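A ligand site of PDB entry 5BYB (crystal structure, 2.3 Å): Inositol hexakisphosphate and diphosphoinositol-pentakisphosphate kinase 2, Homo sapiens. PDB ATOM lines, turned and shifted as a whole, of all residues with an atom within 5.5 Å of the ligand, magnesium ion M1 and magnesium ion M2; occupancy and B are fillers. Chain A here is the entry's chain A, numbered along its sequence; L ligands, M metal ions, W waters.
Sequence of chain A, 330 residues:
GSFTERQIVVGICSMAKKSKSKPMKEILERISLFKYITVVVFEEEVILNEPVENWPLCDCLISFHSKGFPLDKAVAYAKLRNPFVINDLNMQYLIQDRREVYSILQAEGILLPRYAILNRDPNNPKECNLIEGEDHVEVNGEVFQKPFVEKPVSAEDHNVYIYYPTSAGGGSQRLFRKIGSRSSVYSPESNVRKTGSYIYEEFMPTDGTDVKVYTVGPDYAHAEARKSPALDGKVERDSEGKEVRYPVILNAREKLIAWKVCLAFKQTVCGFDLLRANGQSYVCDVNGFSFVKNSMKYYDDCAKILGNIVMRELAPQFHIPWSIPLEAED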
ATOM      1  N   ARG A  98      13.292  18.448  10.327  1.00  0.00           N
ATOM      2  CA  ARG A  98      13.098  19.917  10.327  1.00  0.00           C
ATOM      3  C   ARG A  98      14.394  20.698  10.573  1.00  0.00           C
ATOM      4  O   ARG A  98      14.626  21.733   9.947  1.00  0.00           O
ATOM      5  CB  ARG A  98      12.022  20.342  11.341  1.00  0.00           C
ATOM      6  CG  ARG A  98      10.647  19.784  11.035  1.00  0.00           C
ATOM      7  CD  ARG A  98       9.565  20.487  11.832  1.00  0.00           C
ATOM      8  NE  ARG A  98       8.374  19.643  11.981  1.00  0.00           N
ATOM      9  CZ  ARG A  98       7.368  19.606  11.112  1.00  0.00           C
ATOM     10  NH1 ARG A  98       7.417  20.364  10.029  1.00  0.00           N
ATOM     11  NH2 ARG A  98       6.340  18.799  11.301  1.00  0.00           N
ATOM     12  N   TYR A 102      15.670  23.327   7.812  1.00  0.00           N
ATOM     13  CA  TYR A 102      15.911  24.735   8.150  1.00  0.00           C
ATOM     14  C   TYR A 102      17.353  25.127   7.875  1.00  0.00           C
ATOM     15  O   TYR A 102      17.633  26.234   7.429  1.00  0.00           O
ATOM     16  CB  TYR A 102      15.555  24.995   9.610  1.00  0.00           C
ATOM     17  CG  TYR A 102      14.119  25.400   9.801  1.00  0.00           C
ATOM     18  CD1 TYR A 102      13.113  24.928   8.945  1.00  0.00           C
ATOM     19  CD2 TYR A 102      13.751  26.254  10.845  1.00  0.00           C
ATOM     20  CE1 TYR A 102      11.790  25.312   9.109  1.00  0.00           C
ATOM     21  CE2 TYR A 102      12.426  26.652  11.030  1.00  0.00           C
ATOM     22  CZ  TYR A 102      11.440  26.177  10.161  1.00  0.00           C
ATOM     23  OH  TYR A 102      10.134  26.571  10.334  1.00  0.00           O
ATOM     24  N   PRO A 113      11.414  31.738   9.633  1.00  0.00           N
ATOM     25  CA  PRO A 113      11.282  32.345  10.957  1.00  0.00           C
ATOM     26  C   PRO A 113      12.582  32.261  11.765  1.00  0.00           C
ATOM     27  O   PRO A 113      13.309  31.266  11.640  1.00  0.00           O
ATOM     28  CB  PRO A 113      10.211  31.463  11.624  1.00  0.00           C
ATOM     29  CG  PRO A 113       9.408  30.906  10.498  1.00  0.00           C
ATOM     30  CD  PRO A 113      10.387  30.700   9.372  1.00  0.00           C
ATOM     31  N   VAL A 149       6.109  29.180  18.116  1.00  0.00           N
ATOM     32  CA  VAL A 149       5.673  27.917  17.509  1.00  0.00           C
ATOM     33  C   VAL A 149       6.666  26.827  17.909  1.00  0.00           C
ATOM     34  O   VAL A 149       7.913  27.037  17.942  1.00  0.00           O
ATOM     35  CB  VAL A 149       5.543  28.044  15.963  1.00  0.00           C
ATOM     36  CG1 VAL A 149       4.959  26.762  15.309  1.00  0.00           C
ATOM     37  CG2 VAL A 149       4.710  29.248  15.590  1.00  0.00           C
ATOM     38  N   LYS A 151       7.740  22.927  17.056  1.00  0.00           N
ATOM     39  CA  LYS A 151       7.633  21.846  16.101  1.00  0.00           C
ATOM     40  C   LYS A 151       8.502  20.649  16.471  1.00  0.00           C
ATOM     41  O   LYS A 151       9.668  20.833  16.823  1.00  0.00           O
ATOM     42  CB  LYS A 151       7.979  22.321  14.681  1.00  0.00           C
ATOM     43  CG  LYS A 151       7.141  23.496  14.195  1.00  0.00           C
ATOM     44  CD  LYS A 151       7.429  23.794  12.721  1.00  0.00           C
ATOM     45  CE  LYS A 151       7.070  25.227  12.352  1.00  0.00           C
ATOM     46  NZ  LYS A 151       7.224  25.570  10.908  1.00  0.00           N
ATOM     47  N   ALA A 155       9.968  15.769  10.807  1.00  0.00           N
ATOM     48  CA  ALA A 155       9.073  16.390   9.841  1.00  0.00           C
ATOM     49  C   ALA A 155       7.820  15.563   9.509  1.00  0.00           C
ATOM     50  O   ALA A 155       6.861  16.066   8.885  1.00  0.00           O
ATOM     51  CB  ALA A 155       9.824  16.716   8.560  1.00  0.00           C
ATOM     52  N   ASP A 157       6.081  14.250  11.888  1.00  0.00           N
ATOM     53  CA  ASP A 157       5.259  14.438  13.100  1.00  0.00           C
ATOM     54  C   ASP A 157       4.566  15.787  12.979  1.00  0.00           C
ATOM     55  O   ASP A 157       5.242  16.821  13.102  1.00  0.00           O
ATOM     56  CB  ASP A 157       6.121  14.358  14.379  1.00  0.00           C
ATOM     57  CG  ASP A 157       5.305  14.422  15.663  1.00  0.00           C
ATOM     58  OD1 ASP A 157       4.163  14.942  15.671  1.00  0.00           O
ATOM     59  OD2 ASP A 157       5.834  13.964  16.695  1.00  0.00           O
ATOM     60  N   HIS A 158       3.252  15.789  12.739  1.00  0.00           N
ATOM     61  CA  HIS A 158       2.518  17.043  12.497  1.00  0.00           C
ATOM     62  C   HIS A 158       1.902  17.683  13.743  1.00  0.00           C
ATOM     63  O   HIS A 158       1.102  18.616  13.620  1.00  0.00           O
ATOM     64  CB  HIS A 158       1.480  16.842  11.391  1.00  0.00           C
ATOM     65  CG  HIS A 158       2.072  16.304  10.150  1.00  0.00           C
ATOM     66  ND1 HIS A 158       2.713  17.111   9.226  1.00  0.00           N
ATOM     67  CD2 HIS A 158       2.226  15.033   9.719  1.00  0.00           C
ATOM     68  CE1 HIS A 158       3.182  16.355   8.246  1.00  0.00           C
ATOM     69  NE2 HIS A 158       2.912  15.083   8.532  1.00  0.00           N
ATOM     70  N   VAL A 160       2.260  20.135  15.761  1.00  0.00           N
ATOM     71  CA  VAL A 160       2.811  21.485  15.928  1.00  0.00           C
ATOM     72  C   VAL A 160       1.952  22.299  16.896  1.00  0.00           C
ATOM     73  O   VAL A 160       0.719  22.357  16.742  1.00  0.00           O
ATOM     74  CB  VAL A 160       2.888  22.222  14.571  1.00  0.00           C
ATOM     75  CG1 VAL A 160       3.271  23.665  14.754  1.00  0.00           C
ATOM     76  CG2 VAL A 160       3.852  21.493  13.632  1.00  0.00           C
ATOM     77  N   ILE A 162       1.254  25.992  18.967  1.00  0.00           N
ATOM     78  CA  ILE A 162       1.363  27.432  19.050  1.00  0.00           C
ATOM     79  C   ILE A 162       0.991  27.853  20.491  1.00  0.00           C
ATOM     80  O   ILE A 162      -0.037  27.423  21.014  1.00  0.00           O
ATOM     81  CB  ILE A 162       0.428  28.065  17.999  1.00  0.00           C
ATOM     82  CG1 ILE A 162       0.728  27.384  16.637  1.00  0.00           C
ATOM     83  CG2 ILE A 162       0.558  29.584  17.988  1.00  0.00           C
ATOM     84  CD1 ILE A 162       0.318  28.157  15.402  1.00  0.00           C
ATOM     85  N   LEU A 175      -2.019  21.690  16.604  1.00  0.00           N
ATOM     86  CA  LEU A 175      -2.272  21.268  15.240  1.00  0.00           C
ATOM     87  C   LEU A 175      -2.035  19.759  15.098  1.00  0.00           C
ATOM     88  O   LEU A 175      -1.273  19.164  15.853  1.00  0.00           O
ATOM     89  CB  LEU A 175      -1.366  22.057  14.287  1.00  0.00           C
ATOM     90  CG  LEU A 175      -1.701  23.542  14.139  1.00  0.00           C
ATOM     91  CD1 LEU A 175      -1.606  24.341  15.445  1.00  0.00           C
ATOM     92  CD2 LEU A 175      -0.806  24.151  13.088  1.00  0.00           C
ATOM     93  N   GLU A 201      10.248  28.621  17.216  1.00  0.00           N
ATOM     94  CA  GLU A 201      10.398  29.733  16.303  1.00  0.00           C
ATOM     95  C   GLU A 201       9.361  30.812  16.533  1.00  0.00           C
ATOM     96  O   GLU A 201       8.272  30.558  17.073  1.00  0.00           O
ATOM     97  CB  GLU A 201      10.332  29.253  14.852  1.00  0.00           C
ATOM     98  CG  GLU A 201       9.233  28.262  14.551  1.00  0.00           C
ATOM     99  CD  GLU A 201       9.273  27.795  13.113  1.00  0.00           C
ATOM    100  OE1 GLU A 201       8.626  28.419  12.264  1.00  0.00           O
ATOM    101  OE2 GLU A 201       9.928  26.797  12.829  1.00  0.00           O
ATOM    102  N   GLU A 202       9.715  32.018  16.090  1.00  0.00           N
ATOM    103  CA  GLU A 202       8.816  33.140  16.150  1.00  0.00           C
ATOM    104  C   GLU A 202       7.566  32.900  15.290  1.00  0.00           C
ATOM    105  O   GLU A 202       7.636  32.278  14.201  1.00  0.00           O
ATOM    106  CB  GLU A 202       9.544  34.417  15.729  1.00  0.00           C
ATOM    107  CG  GLU A 202       9.890  34.483  14.255  1.00  0.00           C
ATOM    108  CD  GLU A 202      10.660  35.753  13.862  1.00  0.00           C
ATOM    109  OE1 GLU A 202      10.657  36.688  14.690  1.00  0.00           O
ATOM    110  OE2 GLU A 202      11.275  35.772  12.740  1.00  0.00           O
ATOM    111  N   PHE A 203       6.434  33.345  15.818  1.00  0.00           N
ATOM    112  CA  PHE A 203       5.149  33.224  15.132  1.00  0.00           C
ATOM    113  C   PHE A 203       5.081  34.352  14.112  1.00  0.00           C
ATOM    114  O   PHE A 203       5.231  35.528  14.474  1.00  0.00           O
ATOM    115  CB  PHE A 203       3.998  33.308  16.137  1.00  0.00           C
ATOM    116  CG  PHE A 203       2.632  33.322  15.504  1.00  0.00           C
ATOM    117  CD1 PHE A 203       1.974  32.127  15.214  1.00  0.00           C
ATOM    118  CD2 PHE A 203       1.985  34.528  15.241  1.00  0.00           C
ATOM    119  CE1 PHE A 203       0.705  32.132  14.637  1.00  0.00           C
ATOM    120  CE2 PHE A 203       0.725  34.548  14.650  1.00  0.00           C
ATOM    121  CZ  PHE A 203       0.083  33.351  14.362  1.00  0.00           C
ATOM    122  N   MET A 204       4.861  33.984  12.857  1.00  0.00           N
ATOM    123  CA  MET A 204       4.782  34.963  11.801  1.00  0.00           C
ATOM    124  C   MET A 204       3.309  35.303  11.563  1.00  0.00           C
ATOM    125  O   MET A 204       2.520  34.401  11.160  1.00  0.00           O
ATOM    126  CB  MET A 204       5.451  34.451  10.518  1.00  0.00           C
ATOM    127  CG  MET A 204       6.857  33.868  10.677  1.00  0.00           C
ATOM    128  SD  MET A 204       8.074  34.943  11.474  1.00  0.00           S
ATOM    129  CE  MET A 204       8.154  36.281  10.296  1.00  0.00           C
ATOM    130  N   PRO A 205       2.932  36.585  11.787  1.00  0.00           N
ATOM    131  CA  PRO A 205       1.551  37.009  11.627  1.00  0.00           C
ATOM    132  C   PRO A 205       1.209  37.109  10.149  1.00  0.00           C
ATOM    133  O   PRO A 205       1.740  37.943   9.459  1.00  0.00           O
ATOM    134  CB  PRO A 205       1.544  38.401  12.277  1.00  0.00           C
ATOM    135  CG  PRO A 205       2.916  38.922  12.049  1.00  0.00           C
ATOM    136  CD  PRO A 205       3.829  37.736  12.053  1.00  0.00           C
ATOM    137  N   ASP A 210      -2.196  30.124   4.818  1.00  0.00           N
ATOM    138  CA  ASP A 210      -0.891  29.634   4.444  1.00  0.00           C
ATOM    139  C   ASP A 210      -0.915  29.608   2.943  1.00  0.00           C
ATOM    140  O   ASP A 210      -1.957  29.288   2.350  1.00  0.00           O
ATOM    141  CB  ASP A 210      -0.694  28.177   4.858  1.00  0.00           C
ATOM    142  CG  ASP A 210      -0.911  27.928   6.324  1.00  0.00           C
ATOM    143  OD1 ASP A 210      -0.584  28.802   7.141  1.00  0.00           O
ATOM    144  OD2 ASP A 210      -1.389  26.825   6.680  1.00  0.00           O
ATOM    145  N   LYS A 212       0.637  27.548  -0.083  1.00  0.00           N
ATOM    146  CA  LYS A 212       1.224  26.255  -0.393  1.00  0.00           C
ATOM    147  C   LYS A 212       1.778  26.330  -1.805  1.00  0.00           C
ATOM    148  O   LYS A 212       1.052  26.658  -2.725  1.00  0.00           O
ATOM    149  CB  LYS A 212       0.177  25.137  -0.309  1.00  0.00           C
ATOM    150  CG  LYS A 212      -0.605  25.063   1.010  1.00  0.00           C
ATOM    151  CD  LYS A 212       0.247  24.572   2.177  1.00  0.00           C
ATOM    152  CE  LYS A 212       0.078  23.065   2.448  1.00  0.00           C
ATOM    153  NZ  LYS A 212       1.341  22.294   2.735  1.00  0.00           N
ATOM    154  N   SER A 228      -5.271  28.965   7.674  1.00  0.00           N
ATOM    155  CA  SER A 228      -4.301  28.449   8.601  1.00  0.00           C
ATOM    156  C   SER A 228      -4.996  27.571   9.651  1.00  0.00           C
ATOM    157  O   SER A 228      -5.980  27.978  10.228  1.00  0.00           O
ATOM    158  CB  SER A 228      -3.534  29.560   9.281  1.00  0.00           C
ATOM    159  OG  SER A 228      -2.731  28.964  10.298  1.00  0.00           O
ATOM    160  N   PRO A 229      -4.467  26.352   9.871  1.00  0.00           N
ATOM    161  CA  PRO A 229      -4.957  25.395  10.860  1.00  0.00           C
ATOM    162  C   PRO A 229      -4.976  25.961  12.272  1.00  0.00           C
ATOM    163  O   PRO A 229      -5.837  25.579  13.064  1.00  0.00           O
ATOM    164  CB  PRO A 229      -3.940  24.256  10.781  1.00  0.00           C
ATOM    165  CG  PRO A 229      -3.408  24.322   9.402  1.00  0.00           C
ATOM    166  CD  PRO A 229      -3.319  25.796   9.138  1.00  0.00           C
ATOM    167  N   ALA A 230      -4.049  26.868  12.564  1.00  0.00           N
ATOM    168  CA  ALA A 230      -3.951  27.486  13.882  1.00  0.00           C
ATOM    169  C   ALA A 230      -5.014  28.545  14.153  1.00  0.00           C
ATOM    170  O   ALA A 230      -5.244  28.892  15.309  1.00  0.00           O
ATOM    171  CB  ALA A 230      -2.558  28.074  14.081  1.00  0.00           C
ATOM    172  N   ASP A 273       5.758  25.384   2.105  1.00  0.00           N
ATOM    173  CA  ASP A 273       4.808  26.344   2.639  1.00  0.00           C
ATOM    174  C   ASP A 273       5.438  27.719   2.843  1.00  0.00           C
ATOM    175  O   ASP A 273       6.542  27.825   3.385  1.00  0.00           O
ATOM    176  CB  ASP A 273       4.319  25.874   3.997  1.00  0.00           C
ATOM    177  CG  ASP A 273       3.658  24.500   3.932  1.00  0.00           C
ATOM    178  OD1 ASP A 273       3.357  23.972   2.841  1.00  0.00           O
ATOM    179  OD2 ASP A 273       3.422  23.947   5.000  1.00  0.00           O
ATOM    180  N   LEU A 275       4.766  31.727   4.405  1.00  0.00           N
ATOM    181  CA  LEU A 275       3.985  32.594   5.266  1.00  0.00           C
ATOM    182  C   LEU A 275       4.207  33.999   4.787  1.00  0.00           C
ATOM    183  O   LEU A 275       5.340  34.506   4.852  1.00  0.00           O
ATOM    184  CB  LEU A 275       4.427  32.433   6.732  1.00  0.00           C
ATOM    185  CG  LEU A 275       4.342  31.034   7.378  1.00  0.00           C
ATOM    186  CD1 LEU A 275       4.937  31.088   8.786  1.00  0.00           C
ATOM    187  CD2 LEU A 275       2.930  30.442   7.405  1.00  0.00           C
ATOM    188  N   CYS A 284       8.413  27.908   5.954  1.00  0.00           N
ATOM    189  CA  CYS A 284       8.238  27.261   7.278  1.00  0.00           C
ATOM    190  C   CYS A 284       8.237  25.713   7.230  1.00  0.00           C
ATOM    191  O   CYS A 284       8.239  25.072   8.283  1.00  0.00           O
ATOM    192  CB  CYS A 284       6.968  27.792   7.990  1.00  0.00           C
ATOM    193  SG  CYS A 284       5.389  27.166   7.319  1.00  0.00           S
ATOM    194  N   ASP A 285       8.270  25.147   6.019  1.00  0.00           N
ATOM    195  CA  ASP A 285       8.093  23.702   5.827  1.00  0.00           C
ATOM    196  C   ASP A 285       8.459  23.368   4.373  1.00  0.00           C
ATOM    197  O   ASP A 285       7.952  24.014   3.455  1.00  0.00           O
ATOM    198  CB  ASP A 285       6.611  23.349   6.123  1.00  0.00           C
ATOM    199  CG  ASP A 285       6.309  21.855   6.176  1.00  0.00           C
ATOM    200  OD1 ASP A 285       7.155  20.964   6.338  1.00  0.00           O
ATOM    201  OD2 ASP A 285       5.117  21.555   6.098  1.00  0.00           O
ATOM    202  N   VAL A 286       9.326  22.370   4.166  1.00  0.00           N
ATOM    203  CA  VAL A 286       9.607  21.820   2.829  1.00  0.00           C
ATOM    204  C   VAL A 286       9.301  20.341   2.916  1.00  0.00           C
ATOM    205  O   VAL A 286       9.870  19.626   3.746  1.00  0.00           O
ATOM    206  CB  VAL A 286      11.068  22.004   2.383  1.00  0.00           C
ATOM    207  CG1 VAL A 286      11.244  21.543   0.927  1.00  0.00           C
ATOM    208  CG2 VAL A 286      11.543  23.454   2.577  1.00  0.00           C
ATOM    209  N   ASN A 287       8.388  19.875   2.070  1.00  0.00           N
ATOM    210  CA  ASN A 287       7.879  18.519   2.195  1.00  0.00           C
ATOM    211  C   ASN A 287       8.338  17.582   1.104  1.00  0.00           C
ATOM    212  O   ASN A 287       7.934  16.451   1.107  1.00  0.00           O
ATOM    213  CB  ASN A 287       6.338  18.578   2.201  1.00  0.00           C
ATOM    214  CG  ASN A 287       5.827  19.424   3.348  1.00  0.00           C
ATOM    215  OD1 ASN A 287       6.316  19.241   4.451  1.00  0.00           O
ATOM    216  ND2 ASN A 287       4.944  20.397   3.090  1.00  0.00           N
HETATM  217  P1  LIG L   1       3.859  20.524   8.950  1.00  0.00           P
HETATM  218  O1  LIG L   1       5.170  19.923   8.497  1.00  0.00           O
HETATM  219  O2  LIG L   1       3.125  19.691   9.978  1.00  0.00           O
HETATM  220  O3  LIG L   1       2.934  21.006   7.931  1.00  0.00           O
HETATM  221  P2  LIG L   1       4.458  23.341   9.240  1.00  0.00           P
HETATM  222  O4  LIG L   1       5.837  23.885   9.512  1.00  0.00           O
HETATM  223  O5  LIG L   1       3.816  23.400   7.833  1.00  0.00           O
HETATM  224  O6  LIG L   1       4.424  21.815   9.758  1.00  0.00           O
HETATM  225  O7  LIG L   1       3.437  23.945  10.337  1.00  0.00           O
HETATM  226  C1  LIG L   1       2.030  23.684  10.230  1.00  0.00           C
HETATM  227  C2  LIG L   1       1.239  24.991  10.199  1.00  0.00           C
HETATM  228  O8  LIG L   1       1.475  25.857  11.333  1.00  0.00           O
HETATM  229  C3  LIG L   1       1.578  25.872   9.010  1.00  0.00           C
HETATM  230  O9  LIG L   1       0.802  25.457   7.886  1.00  0.00           O
HETATM  231  C4  LIG L   1       1.189  27.261   9.490  1.00  0.00           C
HETATM  232  O10 LIG L   1      -0.230  27.499   9.387  1.00  0.00           O
HETATM  233  C5  LIG L   1       1.488  27.240  10.958  1.00  0.00           C
HETATM  234  N1  LIG L   1       2.844  27.749  11.236  1.00  0.00           N
HETATM  235  C6  LIG L   1       3.954  27.007  11.166  1.00  0.00           C
HETATM  236  N2  LIG L   1       5.061  27.738  11.463  1.00  0.00           N
HETATM  237  C7  LIG L   1       4.644  28.980  11.734  1.00  0.00           C
HETATM  238  C8  LIG L   1       5.288  30.240  12.147  1.00  0.00           C
HETATM  239  N3  LIG L   1       6.619  30.307  12.313  1.00  0.00           N
HETATM  240  N4  LIG L   1       4.501  31.327  12.344  1.00  0.00           N
HETATM  241  C9  LIG L   1       3.173  31.297  12.183  1.00  0.00           C
HETATM  242  N5  LIG L   1       2.533  30.170  11.806  1.00  0.00           N
HETATM  243  C10 LIG L   1       3.178  28.991  11.582  1.00  0.00           C
HETATM  244 MG    MG M   1       5.531  19.449   6.444  1.00  0.00          MG
HETATM  245 MG    MG M   2       3.054  22.197   6.167  1.00  0.00          MG
HETATM  246  O   HOH W   1      -0.142  30.772  10.905  1.00  0.00           O
HETATM  247  O   HOH W   2       2.513  20.344   5.103  1.00  0.00           O
HETATM  248  O   HOH W   3       6.793  17.962   6.889  1.00  0.00           O
HETATM  249  O   HOH W   4       1.352  20.616  11.430  1.00  0.00           O
HETATM  250  O   HOH W   5       1.289  23.208   6.750  1.00  0.00           O
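Two residues have an atom within 4 Å of magnesium ion M1: Asp 285 and Asn 287.
Water W3 is bound to magnesium ion M1 (2.0 Å). An oxygen (O1) of the ligand binds magnesium ion M1 (2.1 Å). OD1 of Asn 287 is bound to magnesium ion M1. Magnesium ion M1 is bound by OD2 of Asp 285 (2.2 Å). Magnesium ion M1 is bound by the side-chain carboxylate (OD1) of Asp 285 (2.2 Å).
Merely in contact with magnesium ion M2: Lys 212. Of the 27 residues printed, 3 come within 4 Å of magnesium ion M2.
Merely in contact with the ligand: Pro 113 (3.4 Å), Val 149 (3.6 Å), Val 160 (3.9 Å), Leu 175 (3.3 Å), Phe 203 (3.4 Å), Pro 229 (3.5 Å) and Leu 275 (3.5 Å). Hydrophobic or aromatic side chains within 4 Å of the ligand: Pro 113, Val 149, His 158, Val 160, Leu 175, Phe 203, Met 204, Pro 229 and Leu 275. Within 4 Å of the ligand: Arg 98, Pro 113, Val 149, Lys 151, His 158, Val 160, Leu 175, Glu 201, Glu 202, Phe 203, Met 204, Asp 210, Ser 228, Pro 229, Asp 273, Leu 275, Cys 284 and Asp 285. The nearest printed residue that does not touch the ligand is Ala 155 (4.2 Å).
Water W2 lies within hydrogen-bond range of ND2 of Asn 287 and NZ of Lys 212. Water W4 lies within hydrogen-bond range of O2 of the ligand (2.5 Å) and O of His 158 (3.0 Å). Water W1 lies within hydrogen-bond range of N5 of the ligand and OG of Ser 228.
The backbone carbonyl oxygen of Asp 273 sits at hydrogen-bond distance from the backbone NH of Cys 284 (3.2 Å). The backbone carbonyl oxygen (O) of Cys 284 lies within hydrogen-bond range of the side-chain hydroxyl (OH) of Tyr 102 (3.2 Å). The backbone carbonyl oxygen (O) of Glu 201 is in hydrogen-bond range of the backbone NH (N) of Val 149, 2.8 Å away. NZ of Lys 151 lies within hydrogen-bond range of OH of Tyr 102 (3.1 Å). The backbone NH of Leu 175 is in hydrogen-bond range of the backbone carbonyl oxygen of Val 160 (2.8 Å). The side-chain amino group (NZ) of Lys 151 lies within hydrogen-bond range of the backbone carbonyl oxygen (O) of Cys 284, 2.9 Å away. The side-chain amino group of Lys 151 is in salt-bridge range of the side-chain carboxylate of Glu 201. The guanidinium group of Arg 98 lies close to the side-chain carboxylate of Asp 285 (3.7 Å).
Water W5 is bound to magnesium ion M2 (2.1 Å). O3 of the ligand binds magnesium ion M2 (2.1 Å). Magnesium ion M2 is bound by OD2 of Asp 273. The side-chain carboxylate (OD2) of Asp 285 binds magnesium ion M2 (2.2 Å). Magnesium ion M2 is bound by an oxygen (O5) of the ligand, 2.2 Å away. Magnesium ion M2 is bound by water W2, 2.2 Å away.
The backbone carbonyl oxygen (O) of Glu 202 lies within hydrogen-bond range of a nitrogen (N3) of the ligand (2.9 Å). OG of Ser 228 sits at hydrogen-bond distance from O10 of the ligand (3.0 Å). A nitrogen (N4) of the ligand is in hydrogen-bond range of the backbone NH (N) of Met 204, at 2.7 Å. The side-chain carboxylate (OE1) of Glu 201 lies within hydrogen-bond range of a nitrogen (N3) of the ligand (2.8 Å). An oxygen (O2) of the ligand lies within salt-bridge range of the guanidinium group (NH2) of Arg 98, at 3.6 Å. A ring nitrogen (ND1) of His 158 lies within hydrogen-bond range of an oxygen (O2) of the ligand (2.7 Å). O4 of the ligand lies close to O of Cys 284, at 2.9 Å. An oxygen (O10) of the ligand lies within hydrogen-bond range of the side-chain carboxylate of Asp 210. The side-chain amino group (NZ) of Lys 151 is in salt-bridge range of an oxygen (O4) of the ligand, 2.6 Å away.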
